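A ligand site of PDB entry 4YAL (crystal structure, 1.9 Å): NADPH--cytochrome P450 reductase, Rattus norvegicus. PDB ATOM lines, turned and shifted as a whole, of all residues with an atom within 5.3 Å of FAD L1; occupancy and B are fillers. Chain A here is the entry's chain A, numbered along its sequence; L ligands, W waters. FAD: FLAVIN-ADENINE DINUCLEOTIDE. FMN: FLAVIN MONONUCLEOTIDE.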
ATOM      1  N   TYR A  84     -19.275  11.744  -6.042  1.00  0.00           N
ATOM      2  CA  TYR A  84     -19.733  12.852  -6.873  1.00  0.00           C
ATOM      3  C   TYR A  84     -21.199  13.113  -6.583  1.00  0.00           C
ATOM      4  O   TYR A  84     -21.816  12.385  -5.817  1.00  0.00           O
ATOM      5  CB  TYR A  84     -19.537  12.514  -8.356  1.00  0.00           C
ATOM      6  CG  TYR A  84     -19.502  13.741  -9.252  1.00  0.00           C
ATOM      7  CD1 TYR A  84     -18.485  14.683  -9.123  1.00  0.00           C
ATOM      8  CD2 TYR A  84     -20.474  13.962 -10.226  1.00  0.00           C
ATOM      9  CE1 TYR A  84     -18.441  15.817  -9.939  1.00  0.00           C
ATOM     10  CE2 TYR A  84     -20.441  15.094 -11.041  1.00  0.00           C
ATOM     11  CZ  TYR A  84     -19.417  16.016 -10.891  1.00  0.00           C
ATOM     12  OH  TYR A  84     -19.372  17.151 -11.664  1.00  0.00           O
ATOM     13  N   HIS A 263     -26.193  20.983 -16.312  1.00  0.00           N
ATOM     14  CA  HIS A 263     -24.912  21.648 -16.424  1.00  0.00           C
ATOM     15  C   HIS A 263     -24.379  21.500 -17.844  1.00  0.00           C
ATOM     16  O   HIS A 263     -24.683  20.516 -18.520  1.00  0.00           O
ATOM     17  CB  HIS A 263     -23.894  21.044 -15.458  1.00  0.00           C
ATOM     18  CG  HIS A 263     -24.219  21.275 -14.008  1.00  0.00           C
ATOM     19  ND1 HIS A 263     -24.830  20.330 -13.224  1.00  0.00           N
ATOM     20  CD2 HIS A 263     -24.025  22.355 -13.209  1.00  0.00           C
ATOM     21  CE1 HIS A 263     -25.015  20.806 -12.007  1.00  0.00           C
ATOM     22  NE2 HIS A 263     -24.534  22.040 -11.977  1.00  0.00           N
ATOM     23  N   THR A 322      -1.594  24.123 -15.661  1.00  0.00           N
ATOM     24  CA  THR A 322      -1.834  25.232 -14.733  1.00  0.00           C
ATOM     25  C   THR A 322      -2.018  24.871 -13.277  1.00  0.00           C
ATOM     26  O   THR A 322      -1.790  25.713 -12.403  1.00  0.00           O
ATOM     27  CB  THR A 322      -3.064  26.013 -15.176  1.00  0.00           C
ATOM     28  OG1 THR A 322      -4.128  25.101 -15.445  1.00  0.00           O
ATOM     29  CG2 THR A 322      -2.753  26.810 -16.430  1.00  0.00           C
ATOM     30  N   ASN A 323      -2.453  23.653 -12.984  1.00  0.00           N
ATOM     31  CA  ASN A 323      -2.620  23.296 -11.585  1.00  0.00           C
ATOM     32  C   ASN A 323      -1.290  22.841 -11.007  1.00  0.00           C
ATOM     33  O   ASN A 323      -0.400  22.427 -11.745  1.00  0.00           O
ATOM     34  CB  ASN A 323      -3.703  22.230 -11.445  1.00  0.00           C
ATOM     35  CG  ASN A 323      -5.079  22.763 -11.768  1.00  0.00           C
ATOM     36  OD1 ASN A 323      -5.478  23.827 -11.270  1.00  0.00           O
ATOM     37  ND2 ASN A 323      -5.797  22.058 -12.634  1.00  0.00           N
ATOM     38  N   ARG A 368       0.657  28.060  -5.413  1.00  0.00           N
ATOM     39  CA  ARG A 368       0.003  27.776  -6.690  1.00  0.00           C
ATOM     40  C   ARG A 368       0.964  27.828  -7.882  1.00  0.00           C
ATOM     41  O   ARG A 368       0.658  28.418  -8.921  1.00  0.00           O
ATOM     42  CB  ARG A 368      -1.158  28.746  -6.907  1.00  0.00           C
ATOM     43  CG  ARG A 368      -2.284  28.613  -5.881  1.00  0.00           C
ATOM     44  CD  ARG A 368      -3.062  27.330  -6.078  1.00  0.00           C
ATOM     45  NE  ARG A 368      -3.566  27.207  -7.444  1.00  0.00           N
ATOM     46  CZ  ARG A 368      -4.303  26.188  -7.897  1.00  0.00           C
ATOM     47  NH1 ARG A 368      -4.716  26.178  -9.157  1.00  0.00           N
ATOM     48  NH2 ARG A 368      -4.619  25.188  -7.084  1.00  0.00           N
ATOM     49  N   ARG A 398     -14.752  21.829 -17.992  1.00  0.00           N
ATOM     50  CA  ARG A 398     -15.241  22.628 -16.859  1.00  0.00           C
ATOM     51  C   ARG A 398     -16.757  22.667 -16.957  1.00  0.00           C
ATOM     52  O   ARG A 398     -17.310  22.798 -18.058  1.00  0.00           O
ATOM     53  CB  ARG A 398     -14.691  24.062 -16.888  1.00  0.00           C
ATOM     54  CG  ARG A 398     -13.402  24.299 -16.097  1.00  0.00           C
ATOM     55  CD  ARG A 398     -12.197  23.610 -16.725  1.00  0.00           C
ATOM     56  NE  ARG A 398     -10.944  24.063 -16.115  1.00  0.00           N
ATOM     57  CZ  ARG A 398      -9.788  23.410 -16.189  1.00  0.00           C
ATOM     58  NH1 ARG A 398      -8.713  23.912 -15.592  1.00  0.00           N
ATOM     59  NH2 ARG A 398      -9.703  22.250 -16.824  1.00  0.00           N
ATOM     60  N   TYR A 399     -17.428  22.565 -15.815  1.00  0.00           N
ATOM     61  CA  TYR A 399     -18.886  22.577 -15.759  1.00  0.00           C
ATOM     62  C   TYR A 399     -19.460  23.938 -15.351  1.00  0.00           C
ATOM     63  O   TYR A 399     -18.903  24.624 -14.497  1.00  0.00           O
ATOM     64  CB  TYR A 399     -19.376  21.535 -14.738  1.00  0.00           C
ATOM     65  CG  TYR A 399     -19.059  20.101 -15.095  1.00  0.00           C
ATOM     66  CD1 TYR A 399     -19.836  19.410 -16.015  1.00  0.00           C
ATOM     67  CD2 TYR A 399     -18.003  19.430 -14.483  1.00  0.00           C
ATOM     68  CE1 TYR A 399     -19.571  18.066 -16.315  1.00  0.00           C
ATOM     69  CE2 TYR A 399     -17.737  18.086 -14.769  1.00  0.00           C
ATOM     70  CZ  TYR A 399     -18.530  17.420 -15.689  1.00  0.00           C
ATOM     71  OH  TYR A 399     -18.294  16.083 -15.931  1.00  0.00           O
ATOM     72  N   TYR A 400     -20.592  24.298 -15.966  1.00  0.00           N
ATOM     73  CA  TYR A 400     -21.278  25.548 -15.669  1.00  0.00           C
ATOM     74  C   TYR A 400     -22.763  25.240 -15.541  1.00  0.00           C
ATOM     75  O   TYR A 400     -23.291  24.360 -16.236  1.00  0.00           O
ATOM     76  CB  TYR A 400     -21.020  26.589 -16.764  1.00  0.00           C
ATOM     77  CG  TYR A 400     -19.581  27.025 -16.772  1.00  0.00           C
ATOM     78  CD1 TYR A 400     -19.114  27.958 -15.842  1.00  0.00           C
ATOM     79  CD2 TYR A 400     -18.641  26.396 -17.600  1.00  0.00           C
ATOM     80  CE1 TYR A 400     -17.761  28.235 -15.708  1.00  0.00           C
ATOM     81  CE2 TYR A 400     -17.285  26.659 -17.479  1.00  0.00           C
ATOM     82  CZ  TYR A 400     -16.853  27.569 -16.533  1.00  0.00           C
ATOM     83  OH  TYR A 400     -15.497  27.766 -16.361  1.00  0.00           O
ATOM     84  N   SER A 401     -23.439  25.945 -14.651  1.00  0.00           N
ATOM     85  CA  SER A 401     -24.858  25.720 -14.436  1.00  0.00           C
ATOM     86  C   SER A 401     -25.634  26.481 -15.512  1.00  0.00           C
ATOM     87  O   SER A 401     -25.621  27.710 -15.542  1.00  0.00           O
ATOM     88  CB  SER A 401     -25.257  26.224 -13.046  1.00  0.00           C
ATOM     89  OG  SER A 401     -24.413  25.619 -12.070  1.00  0.00           O
ATOM     90  N   CYS A 416     -23.286  31.758 -16.896  1.00  0.00           N
ATOM     91  CA  CYS A 416     -23.021  32.901 -16.031  1.00  0.00           C
ATOM     92  C   CYS A 416     -21.778  32.507 -15.245  1.00  0.00           C
ATOM     93  O   CYS A 416     -21.813  31.579 -14.448  1.00  0.00           O
ATOM     94  CB  CYS A 416     -24.193  33.136 -15.069  1.00  0.00           C
ATOM     95  SG  CYS A 416     -23.877  34.442 -13.842  1.00  0.00           S
ATOM     96  N   ALA A 417     -20.670  33.220 -15.455  1.00  0.00           N
ATOM     97  CA  ALA A 417     -19.437  32.881 -14.782  1.00  0.00           C
ATOM     98  C   ALA A 417     -18.579  34.062 -14.382  1.00  0.00           C
ATOM     99  O   ALA A 417     -18.694  35.144 -14.947  1.00  0.00           O
ATOM    100  CB  ALA A 417     -18.617  31.943 -15.667  1.00  0.00           C
ATOM    101  N   VAL A 418     -17.742  33.850 -13.387  1.00  0.00           N
ATOM    102  CA  VAL A 418     -16.820  34.873 -12.943  1.00  0.00           C
ATOM    103  C   VAL A 418     -15.449  34.446 -13.472  1.00  0.00           C
ATOM    104  O   VAL A 418     -15.051  33.287 -13.345  1.00  0.00           O
ATOM    105  CB  VAL A 418     -16.781  34.995 -11.397  1.00  0.00           C
ATOM    106  CG1 VAL A 418     -16.432  33.660 -10.760  1.00  0.00           C
ATOM    107  CG2 VAL A 418     -15.786  36.087 -10.994  1.00  0.00           C
ATOM    108  N   VAL A 420     -11.603  33.894 -13.598  1.00  0.00           N
ATOM    109  CA  VAL A 420     -10.612  33.657 -12.561  1.00  0.00           C
ATOM    110  C   VAL A 420      -9.273  34.282 -12.923  1.00  0.00           C
ATOM    111  O   VAL A 420      -8.705  34.001 -13.973  1.00  0.00           O
ATOM    112  CB  VAL A 420     -10.426  32.145 -12.308  1.00  0.00           C
ATOM    113  CG1 VAL A 420      -9.325  31.920 -11.277  1.00  0.00           C
ATOM    114  CG2 VAL A 420     -11.731  31.544 -11.806  1.00  0.00           C
ATOM    115  N   TYR A 422      -5.933  35.870 -10.390  1.00  0.00           N
ATOM    116  CA  TYR A 422      -5.474  36.279  -9.078  1.00  0.00           C
ATOM    117  C   TYR A 422      -3.958  36.283  -8.953  1.00  0.00           C
ATOM    118  O   TYR A 422      -3.251  35.610  -9.710  1.00  0.00           O
ATOM    119  CB  TYR A 422      -6.041  35.348  -8.013  1.00  0.00           C
ATOM    120  CG  TYR A 422      -5.642  33.909  -8.204  1.00  0.00           C
ATOM    121  CD1 TYR A 422      -6.283  33.091  -9.142  1.00  0.00           C
ATOM    122  CD2 TYR A 422      -4.571  33.367  -7.490  1.00  0.00           C
ATOM    123  CE1 TYR A 422      -5.866  31.779  -9.359  1.00  0.00           C
ATOM    124  CE2 TYR A 422      -4.142  32.051  -7.700  1.00  0.00           C
ATOM    125  CZ  TYR A 422      -4.792  31.268  -8.632  1.00  0.00           C
ATOM    126  OH  TYR A 422      -4.360  29.975  -8.850  1.00  0.00           O
ATOM    127  N   LYS A 431      -4.197  32.589 -14.177  1.00  0.00           N
ATOM    128  CA  LYS A 431      -5.419  32.785 -14.932  1.00  0.00           C
ATOM    129  C   LYS A 431      -6.223  31.496 -15.057  1.00  0.00           C
ATOM    130  O   LYS A 431      -5.673  30.444 -15.393  1.00  0.00           O
ATOM    131  CB  LYS A 431      -5.096  33.298 -16.328  1.00  0.00           C
ATOM    132  CG  LYS A 431      -4.291  34.586 -16.374  1.00  0.00           C
ATOM    133  CD  LYS A 431      -5.156  35.805 -16.081  1.00  0.00           C
ATOM    134  CE  LYS A 431      -6.223  35.971 -17.148  1.00  0.00           C
ATOM    135  NZ  LYS A 431      -5.606  36.116 -18.502  1.00  0.00           N
ATOM    136  N   GLY A 432      -7.532  31.578 -14.812  1.00  0.00           N
ATOM    137  CA  GLY A 432      -8.388  30.414 -14.930  1.00  0.00           C
ATOM    138  C   GLY A 432      -8.388  29.961 -16.379  1.00  0.00           C
ATOM    139  O   GLY A 432      -8.589  30.776 -17.280  1.00  0.00           O
ATOM    140  N   VAL A 433      -8.174  28.670 -16.614  1.00  0.00           N
ATOM    141  CA  VAL A 433      -8.123  28.157 -17.978  1.00  0.00           C
ATOM    142  C   VAL A 433      -9.393  28.362 -18.794  1.00  0.00           C
ATOM    143  O   VAL A 433      -9.383  29.011 -19.845  1.00  0.00           O
ATOM    144  CB  VAL A 433      -7.776  26.640 -17.988  1.00  0.00           C
ATOM    145  CG1 VAL A 433      -7.750  26.128 -19.429  1.00  0.00           C
ATOM    146  CG2 VAL A 433      -6.424  26.404 -17.310  1.00  0.00           C
ATOM    147  N   ALA A 434     -10.498  27.783 -18.318  1.00  0.00           N
ATOM    148  CA  ALA A 434     -11.776  27.885 -19.018  1.00  0.00           C
ATOM    149  C   ALA A 434     -12.354  29.284 -19.064  1.00  0.00           C
ATOM    150  O   ALA A 434     -12.861  29.727 -20.110  1.00  0.00           O
ATOM    151  CB  ALA A 434     -12.781  26.910 -18.396  1.00  0.00           C
ATOM    152  N   THR A 435     -12.297  30.004 -17.944  1.00  0.00           N
ATOM    153  CA  THR A 435     -12.868  31.347 -17.918  1.00  0.00           C
ATOM    154  C   THR A 435     -12.073  32.368 -18.743  1.00  0.00           C
ATOM    155  O   THR A 435     -12.666  33.246 -19.370  1.00  0.00           O
ATOM    156  CB  THR A 435     -13.070  31.865 -16.461  1.00  0.00           C
ATOM    157  OG1 THR A 435     -11.847  31.779 -15.730  1.00  0.00           O
ATOM    158  CG2 THR A 435     -14.146  31.019 -15.767  1.00  0.00           C
ATOM    159  N   SER A 436     -10.752  32.248 -18.788  1.00  0.00           N
ATOM    160  CA  SER A 436      -9.966  33.193 -19.582  1.00  0.00           C
ATOM    161  C   SER A 436     -10.289  32.949 -21.046  1.00  0.00           C
ATOM    162  O   SER A 436     -10.450  33.878 -21.825  1.00  0.00           O
ATOM    163  CB  SER A 436      -8.459  32.978 -19.352  1.00  0.00           C
ATOM    164  OG  SER A 436      -8.123  33.305 -18.010  1.00  0.00           O
ATOM    165  N   THR A 479     -22.639  34.350  -8.494  1.00  0.00           N
ATOM    166  CA  THR A 479     -22.877  33.517  -9.679  1.00  0.00           C
ATOM    167  C   THR A 479     -23.802  32.362  -9.348  1.00  0.00           C
ATOM    168  O   THR A 479     -24.168  31.573 -10.216  1.00  0.00           O
ATOM    169  CB  THR A 479     -21.565  32.951 -10.238  1.00  0.00           C
ATOM    170  OG1 THR A 479     -20.883  32.224  -9.201  1.00  0.00           O
ATOM    171  CG2 THR A 479     -20.673  34.066 -10.765  1.00  0.00           C
ATOM    172  N   ALA A 482     -27.087  31.649 -11.346  1.00  0.00           N
ATOM    173  CA  ALA A 482     -27.106  30.981 -12.639  1.00  0.00           C
ATOM    174  C   ALA A 482     -28.275  30.055 -13.001  1.00  0.00           C
ATOM    175  O   ALA A 482     -29.012  30.330 -13.953  1.00  0.00           O
ATOM    176  CB  ALA A 482     -25.781  30.239 -12.861  1.00  0.00           C
ATOM    177  N   ASP A 619     -26.523  22.895  -5.703  1.00  0.00           N
ATOM    178  CA  ASP A 619     -25.728  23.065  -6.903  1.00  0.00           C
ATOM    179  C   ASP A 619     -24.639  24.007  -6.431  1.00  0.00           C
ATOM    180  O   ASP A 619     -24.620  25.192  -6.744  1.00  0.00           O
ATOM    181  CB  ASP A 619     -26.526  23.694  -8.052  1.00  0.00           C
ATOM    182  CG  ASP A 619     -25.709  23.803  -9.330  1.00  0.00           C
ATOM    183  OD1 ASP A 619     -24.695  23.084  -9.466  1.00  0.00           O
ATOM    184  OD2 ASP A 619     -26.077  24.590 -10.222  1.00  0.00           O
ATOM    185  N   TRP A 621     -20.347  24.543  -5.672  1.00  0.00           N
ATOM    186  CA  TRP A 621     -19.043  24.114  -6.113  1.00  0.00           C
ATOM    187  C   TRP A 621     -17.946  24.879  -5.403  1.00  0.00           C
ATOM    188  O   TRP A 621     -18.215  25.818  -4.654  1.00  0.00           O
ATOM    189  CB  TRP A 621     -18.927  24.318  -7.640  1.00  0.00           C
ATOM    190  CG  TRP A 621     -19.103  25.751  -8.069  1.00  0.00           C
ATOM    191  CD1 TRP A 621     -18.133  26.708  -8.150  1.00  0.00           C
ATOM    192  CD2 TRP A 621     -20.334  26.386  -8.465  1.00  0.00           C
ATOM    193  NE1 TRP A 621     -18.683  27.905  -8.575  1.00  0.00           N
ATOM    194  CE2 TRP A 621     -20.024  27.726  -8.776  1.00  0.00           C
ATOM    195  CE3 TRP A 621     -21.657  25.949  -8.604  1.00  0.00           C
ATOM    196  CZ2 TRP A 621     -20.999  28.646  -9.207  1.00  0.00           C
ATOM    197  CZ3 TRP A 621     -22.630  26.862  -9.028  1.00  0.00           C
ATOM    198  CH2 TRP A 621     -22.287  28.196  -9.327  1.00  0.00           C
ATOM    199  N   SER A 622     -16.712  24.449  -5.642  1.00  0.00           N
ATOM    200  CA  SER A 622     -15.531  25.059  -5.060  1.00  0.00           C
ATOM    201  C   SER A 622     -15.642  25.075  -3.539  1.00  0.00           C
ATOM    202  O   SER A 622     -15.671  26.170  -2.941  1.00  0.00           O
ATOM    203  CB  SER A 622     -15.350  26.487  -5.586  1.00  0.00           C
ATOM    204  OG  SER A 622     -14.054  26.984  -5.298  1.00  0.00           O
ATOM    205  OXT SER A 622     -15.726  23.965  -2.955  1.00  0.00           O
HETATM  206  PA  FAD L   1      -9.024  26.873 -13.246  1.00  0.00           P
HETATM  207  O1A FAD L   1      -7.868  27.037 -14.154  1.00  0.00           O
HETATM  208  O2A FAD L   1      -9.703  25.545 -13.178  1.00  0.00           O
HETATM  209  O5B FAD L   1      -8.574  27.275 -11.756  1.00  0.00           O
HETATM  210  C5B FAD L   1      -9.443  27.004 -10.656  1.00  0.00           C
HETATM  211  C4B FAD L   1      -8.606  26.978  -9.375  1.00  0.00           C
HETATM  212  O4B FAD L   1      -7.956  28.242  -9.171  1.00  0.00           O
HETATM  213  C3B FAD L   1      -9.491  26.880  -8.150  1.00  0.00           C
HETATM  214  O3B FAD L   1      -9.916  25.509  -8.002  1.00  0.00           O
HETATM  215  C2B FAD L   1      -8.445  27.197  -7.101  1.00  0.00           C
HETATM  216  O2B FAD L   1      -7.634  26.028  -6.853  1.00  0.00           O
HETATM  217  C1B FAD L   1      -7.602  28.268  -7.780  1.00  0.00           C
HETATM  218  N9A FAD L   1      -7.954  29.628  -7.299  1.00  0.00           N
HETATM  219  C8A FAD L   1      -9.090  30.441  -7.769  1.00  0.00           C
HETATM  220  N7A FAD L   1      -8.867  31.682  -7.010  1.00  0.00           N
HETATM  221  C5A FAD L   1      -7.817  31.522  -6.212  1.00  0.00           C
HETATM  222  C6A FAD L   1      -7.276  32.386  -5.369  1.00  0.00           C
HETATM  223  N6A FAD L   1      -7.797  33.610  -5.371  1.00  0.00           N
HETATM  224  N1A FAD L   1      -6.196  32.095  -4.632  1.00  0.00           N
HETATM  225  C2A FAD L   1      -5.619  30.826  -4.760  1.00  0.00           C
HETATM  226  N3A FAD L   1      -6.208  29.934  -5.656  1.00  0.00           N
HETATM  227  C4A FAD L   1      -7.296  30.304  -6.358  1.00  0.00           C
HETATM  228  N1  FAD L   1     -18.489  28.487 -12.056  1.00  0.00           N
HETATM  229  C2  FAD L   1     -19.161  29.631 -12.508  1.00  0.00           C
HETATM  230  O2  FAD L   1     -18.570  30.711 -12.516  1.00  0.00           O
HETATM  231  N3  FAD L   1     -20.502  29.530 -12.888  1.00  0.00           N
HETATM  232  C4  FAD L   1     -21.177  28.313 -12.802  1.00  0.00           C
HETATM  233  O4  FAD L   1     -22.340  28.236 -13.213  1.00  0.00           O
HETATM  234  C4X FAD L   1     -20.518  27.181 -12.335  1.00  0.00           C
HETATM  235  N5  FAD L   1     -21.185  26.056 -12.067  1.00  0.00           N
HETATM  236  C5X FAD L   1     -20.529  24.973 -11.622  1.00  0.00           C
HETATM  237  C6  FAD L   1     -21.204  23.772 -11.465  1.00  0.00           C
HETATM  238  C7  FAD L   1     -20.514  22.617 -11.099  1.00  0.00           C
HETATM  239  C7M FAD L   1     -21.202  21.419 -10.977  1.00  0.00           C
HETATM  240  C8  FAD L   1     -19.141  22.673 -10.896  1.00  0.00           C
HETATM  241  C8M FAD L   1     -18.434  21.530 -10.552  1.00  0.00           C
HETATM  242  C9  FAD L   1     -18.456  23.877 -11.054  1.00  0.00           C
HETATM  243  C9A FAD L   1     -19.145  25.017 -11.449  1.00  0.00           C
HETATM  244  N10 FAD L   1     -18.490  26.154 -11.702  1.00  0.00           N
HETATM  245  C10 FAD L   1     -19.176  27.275 -11.962  1.00  0.00           C
HETATM  246  C1' FAD L   1     -17.018  26.258 -11.541  1.00  0.00           C
HETATM  247  C2' FAD L   1     -16.357  26.026 -12.909  1.00  0.00           C
HETATM  248  O2' FAD L   1     -16.614  24.678 -13.323  1.00  0.00           O
HETATM  249  C3' FAD L   1     -14.843  26.263 -12.874  1.00  0.00           C
HETATM  250  O3' FAD L   1     -14.269  25.524 -11.789  1.00  0.00           O
HETATM  251  C4' FAD L   1     -14.524  27.756 -12.708  1.00  0.00           C
HETATM  252  O4' FAD L   1     -15.161  28.508 -13.748  1.00  0.00           O
HETATM  253  C5' FAD L   1     -13.007  27.948 -12.800  1.00  0.00           C
HETATM  254  O5' FAD L   1     -12.529  27.343 -14.000  1.00  0.00           O
HETATM  255  P   FAD L   1     -11.210  27.871 -14.755  1.00  0.00           P
HETATM  256  O1P FAD L   1     -11.455  29.227 -15.278  1.00  0.00           O
HETATM  257  O2P FAD L   1     -10.789  26.816 -15.715  1.00  0.00           O
HETATM  258  O3P FAD L   1     -10.118  27.997 -13.577  1.00  0.00           O
HETATM  259  N1  FMN L   2     -16.939  14.461  -2.109  1.00  0.00           N
HETATM  260  C2  FMN L   2     -17.582  13.765  -1.151  1.00  0.00           C
HETATM  261  O2  FMN L   2     -16.967  13.233  -0.222  1.00  0.00           O
HETATM  262  N3  FMN L   2     -18.960  13.665  -1.268  1.00  0.00           N
HETATM  263  C4  FMN L   2     -19.769  14.213  -2.265  1.00  0.00           C
HETATM  264  O4  FMN L   2     -20.978  13.991  -2.153  1.00  0.00           O
HETATM  265  C4A FMN L   2     -19.113  14.970  -3.267  1.00  0.00           C
HETATM  266  N5  FMN L   2     -19.901  15.552  -4.281  1.00  0.00           N
HETATM  267  C5A FMN L   2     -19.185  16.296  -5.215  1.00  0.00           C
HETATM  268  C6  FMN L   2     -19.977  16.929  -6.237  1.00  0.00           C
HETATM  269  C7  FMN L   2     -19.372  17.724  -7.244  1.00  0.00           C
HETATM  270  C7M FMN L   2     -20.347  18.345  -8.277  1.00  0.00           C
HETATM  271  C8  FMN L   2     -17.884  17.924  -7.278  1.00  0.00           C
HETATM  272  C8M FMN L   2     -17.189  18.669  -8.204  1.00  0.00           C
HETATM  273  C9  FMN L   2     -17.112  17.315  -6.298  1.00  0.00           C
HETATM  274  C9A FMN L   2     -17.717  16.491  -5.248  1.00  0.00           C
HETATM  275  N10 FMN L   2     -16.965  15.827  -4.159  1.00  0.00           N
HETATM  276  C10 FMN L   2     -17.677  15.049  -3.132  1.00  0.00           C
HETATM  277  C1' FMN L   2     -15.517  15.960  -4.090  1.00  0.00           C
HETATM  278  C2' FMN L   2     -14.727  14.906  -4.935  1.00  0.00           C
HETATM  279  O2' FMN L   2     -15.083  13.541  -4.465  1.00  0.00           O
HETATM  280  C3' FMN L   2     -13.229  15.146  -4.793  1.00  0.00           C
HETATM  281  O3' FMN L   2     -12.960  16.481  -5.293  1.00  0.00           O
HETATM  282  C4' FMN L   2     -12.480  14.053  -5.607  1.00  0.00           C
HETATM  283  O4' FMN L   2     -11.089  14.414  -5.349  1.00  0.00           O
HETATM  284  C5' FMN L   2     -12.673  14.141  -7.107  1.00  0.00           C
HETATM  285  O5' FMN L   2     -11.988  13.039  -7.825  1.00  0.00           O
HETATM  286  P   FMN L   2     -11.988  12.840  -9.386  1.00  0.00           P
HETATM  287  O1P FMN L   2     -11.200  13.934 -10.027  1.00  0.00           O
HETATM  288  O2P FMN L   2     -13.490  12.646  -9.748  1.00  0.00           O
HETATM  289  O3P FMN L   2     -11.141  11.486  -9.518  1.00  0.00           O
HETATM  290  O   HOH W   1     -11.151  33.347  -7.978  1.00  0.00           O
HETATM  291  O   HOH W   2      -5.195  28.558 -13.404  1.00  0.00           O
HETATM  292  O   HOH W   3     -13.554  26.597  -9.189  1.00  0.00           O
HETATM  293  O   HOH W   4      -5.563  28.492 -10.634  1.00  0.00           O
HETATM  294  O   HOH W   5      -5.911  25.217 -13.611  1.00  0.00           O
HETATM  295  O   HOH W   6     -15.633  22.185 -13.329  1.00  0.00           O
HETATM  296  O   HOH W   7     -15.967  30.723 -12.512  1.00  0.00           O
HETATM  297  O   HOH W   8      -8.169  23.264  -9.365  1.00  0.00           O
HETATM  298  O   HOH W   9      -8.605  23.123 -12.115  1.00  0.00           O
HETATM  299  O   HOH W  10     -11.889  24.215 -12.549  1.00  0.00           O
HETATM  300  O   HOH W  11     -23.433  29.244 -15.603  1.00  0.00           O
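Water W6 bridges O2' of FAD L1 (2.7 Å) and N of Tyr 399 (3.1 Å).
Water W5 lies within hydrogen-bond range of the side-chain hydroxyl (OG1) of Thr 322 (2.6 Å), an oxygen (O1A) of FAD L1 (2.7 Å) and the side-chain amide oxygen (OD1) of Asn 323 (2.8 Å).
Water W4 lies within hydrogen-bond range of the side-chain hydroxyl (OH) of Tyr 422 (2.6 Å), an oxygen (O4B) of FAD L1 (2.8 Å) and the guanidinium group (NH1) of Arg 368 (2.9 Å).
Water W9 bridges O2A of FAD L1 (2.9 Å) and ND2 of Asn 323 (3.0 Å).
Water W8 lies within hydrogen-bond range of an oxygen (O3B) of FAD L1 (3.2 Å) and the side-chain amide oxygen of Asn 323 (3.3 Å).
Water W2 lies within hydrogen-bond range of the backbone carbonyl oxygen (O) of Lys 431 and an oxygen (O1A) of FAD L1.
The backbone carbonyl oxygen (O) of Cys 416 sits at hydrogen-bond distance from a nitrogen (N3) of FAD L1 (2.9 Å).
N of Val 433 is in hydrogen-bond range of O1A of FAD L1 (3.0 Å).
An oxygen (O2) of FAD L1 lies within hydrogen-bond range of the backbone NH (N) of Val 418 (3.4 Å).
NE of Arg 398 lies within salt-bridge range of O2P of FAD L1 (2.8 Å).
An oxygen (O2') of FAD L1 is in hydrogen-bond range of the backbone carbonyl oxygen (O) of Tyr 399, 2.6 Å away.
The guanidinium group of Arg 368 lies within hydrogen-bond range of an oxygen (O2B) of FAD L1 (3.1 Å).
An oxygen (O4) of FAD L1 sits at hydrogen-bond distance from the backbone NH (N) of Ser 401 (2.9 Å).
O2' of FAD L1 is in hydrogen-bond range of N of Tyr 399.
N of Ala 434 is in hydrogen-bond range of O2P of FAD L1 (2.8 Å).
N5 of FAD L1 sits at hydrogen-bond distance from OG of Ser 401 (3.3 Å).
An oxygen (O1P) of FAD L1 lies within hydrogen-bond range of the backbone NH (N) of Thr 435, at 2.9 Å.
OH of Tyr 400 sits at hydrogen-bond distance from O4' of FAD L1, at 2.7 Å.
O1P of FAD L1 lies within hydrogen-bond range of OG1 of Thr 435, at 2.6 Å.
The guanidinium group of Arg 368 is in hydrogen-bond range of the side-chain hydroxyl of Tyr 422, 3.2 Å away.
The side-chain hydroxyl of Thr 435 is in hydrogen-bond range of the backbone NH of Val 420, at 3.0 Å.
O of Val 420 lies within hydrogen-bond range of N of Gly 432 (2.8 Å).
The side-chain hydroxyl (OG) of Ser 401 lies within hydrogen-bond range of the side-chain carboxylate (OD2) of Asp 619, at 2.7 Å.
NH1 of Arg 368 lies within hydrogen-bond range of OD1 of Asn 323 (3.3 Å).
O of Gly 432 sits at hydrogen-bond distance from OG of Ser 436, at 2.7 Å.
The side-chain carboxylate (OD1) of Asp 619 is in hydrogen-bond range of a ring nitrogen (NE2) of His 263, at 2.7 Å.
His 263 touches FAD L1.
Ala 417 touches FAD L1.
CG1 of Val 420 touches C8A of FAD L1, at 3.8 Å.
Tyr 422 touches FAD L1 (CE2 to C2A, 3.5 Å).
Gly 432 touches FAD L1 (CA to O3P, 3.3 Å).
Ala 482 touches FAD L1.
Trp 621 touches FAD L1 (CE2 to C10, 3.3 Å).
The nearest printed residue that does not touch FAD L1 is Asp 619 (4.1 Å).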
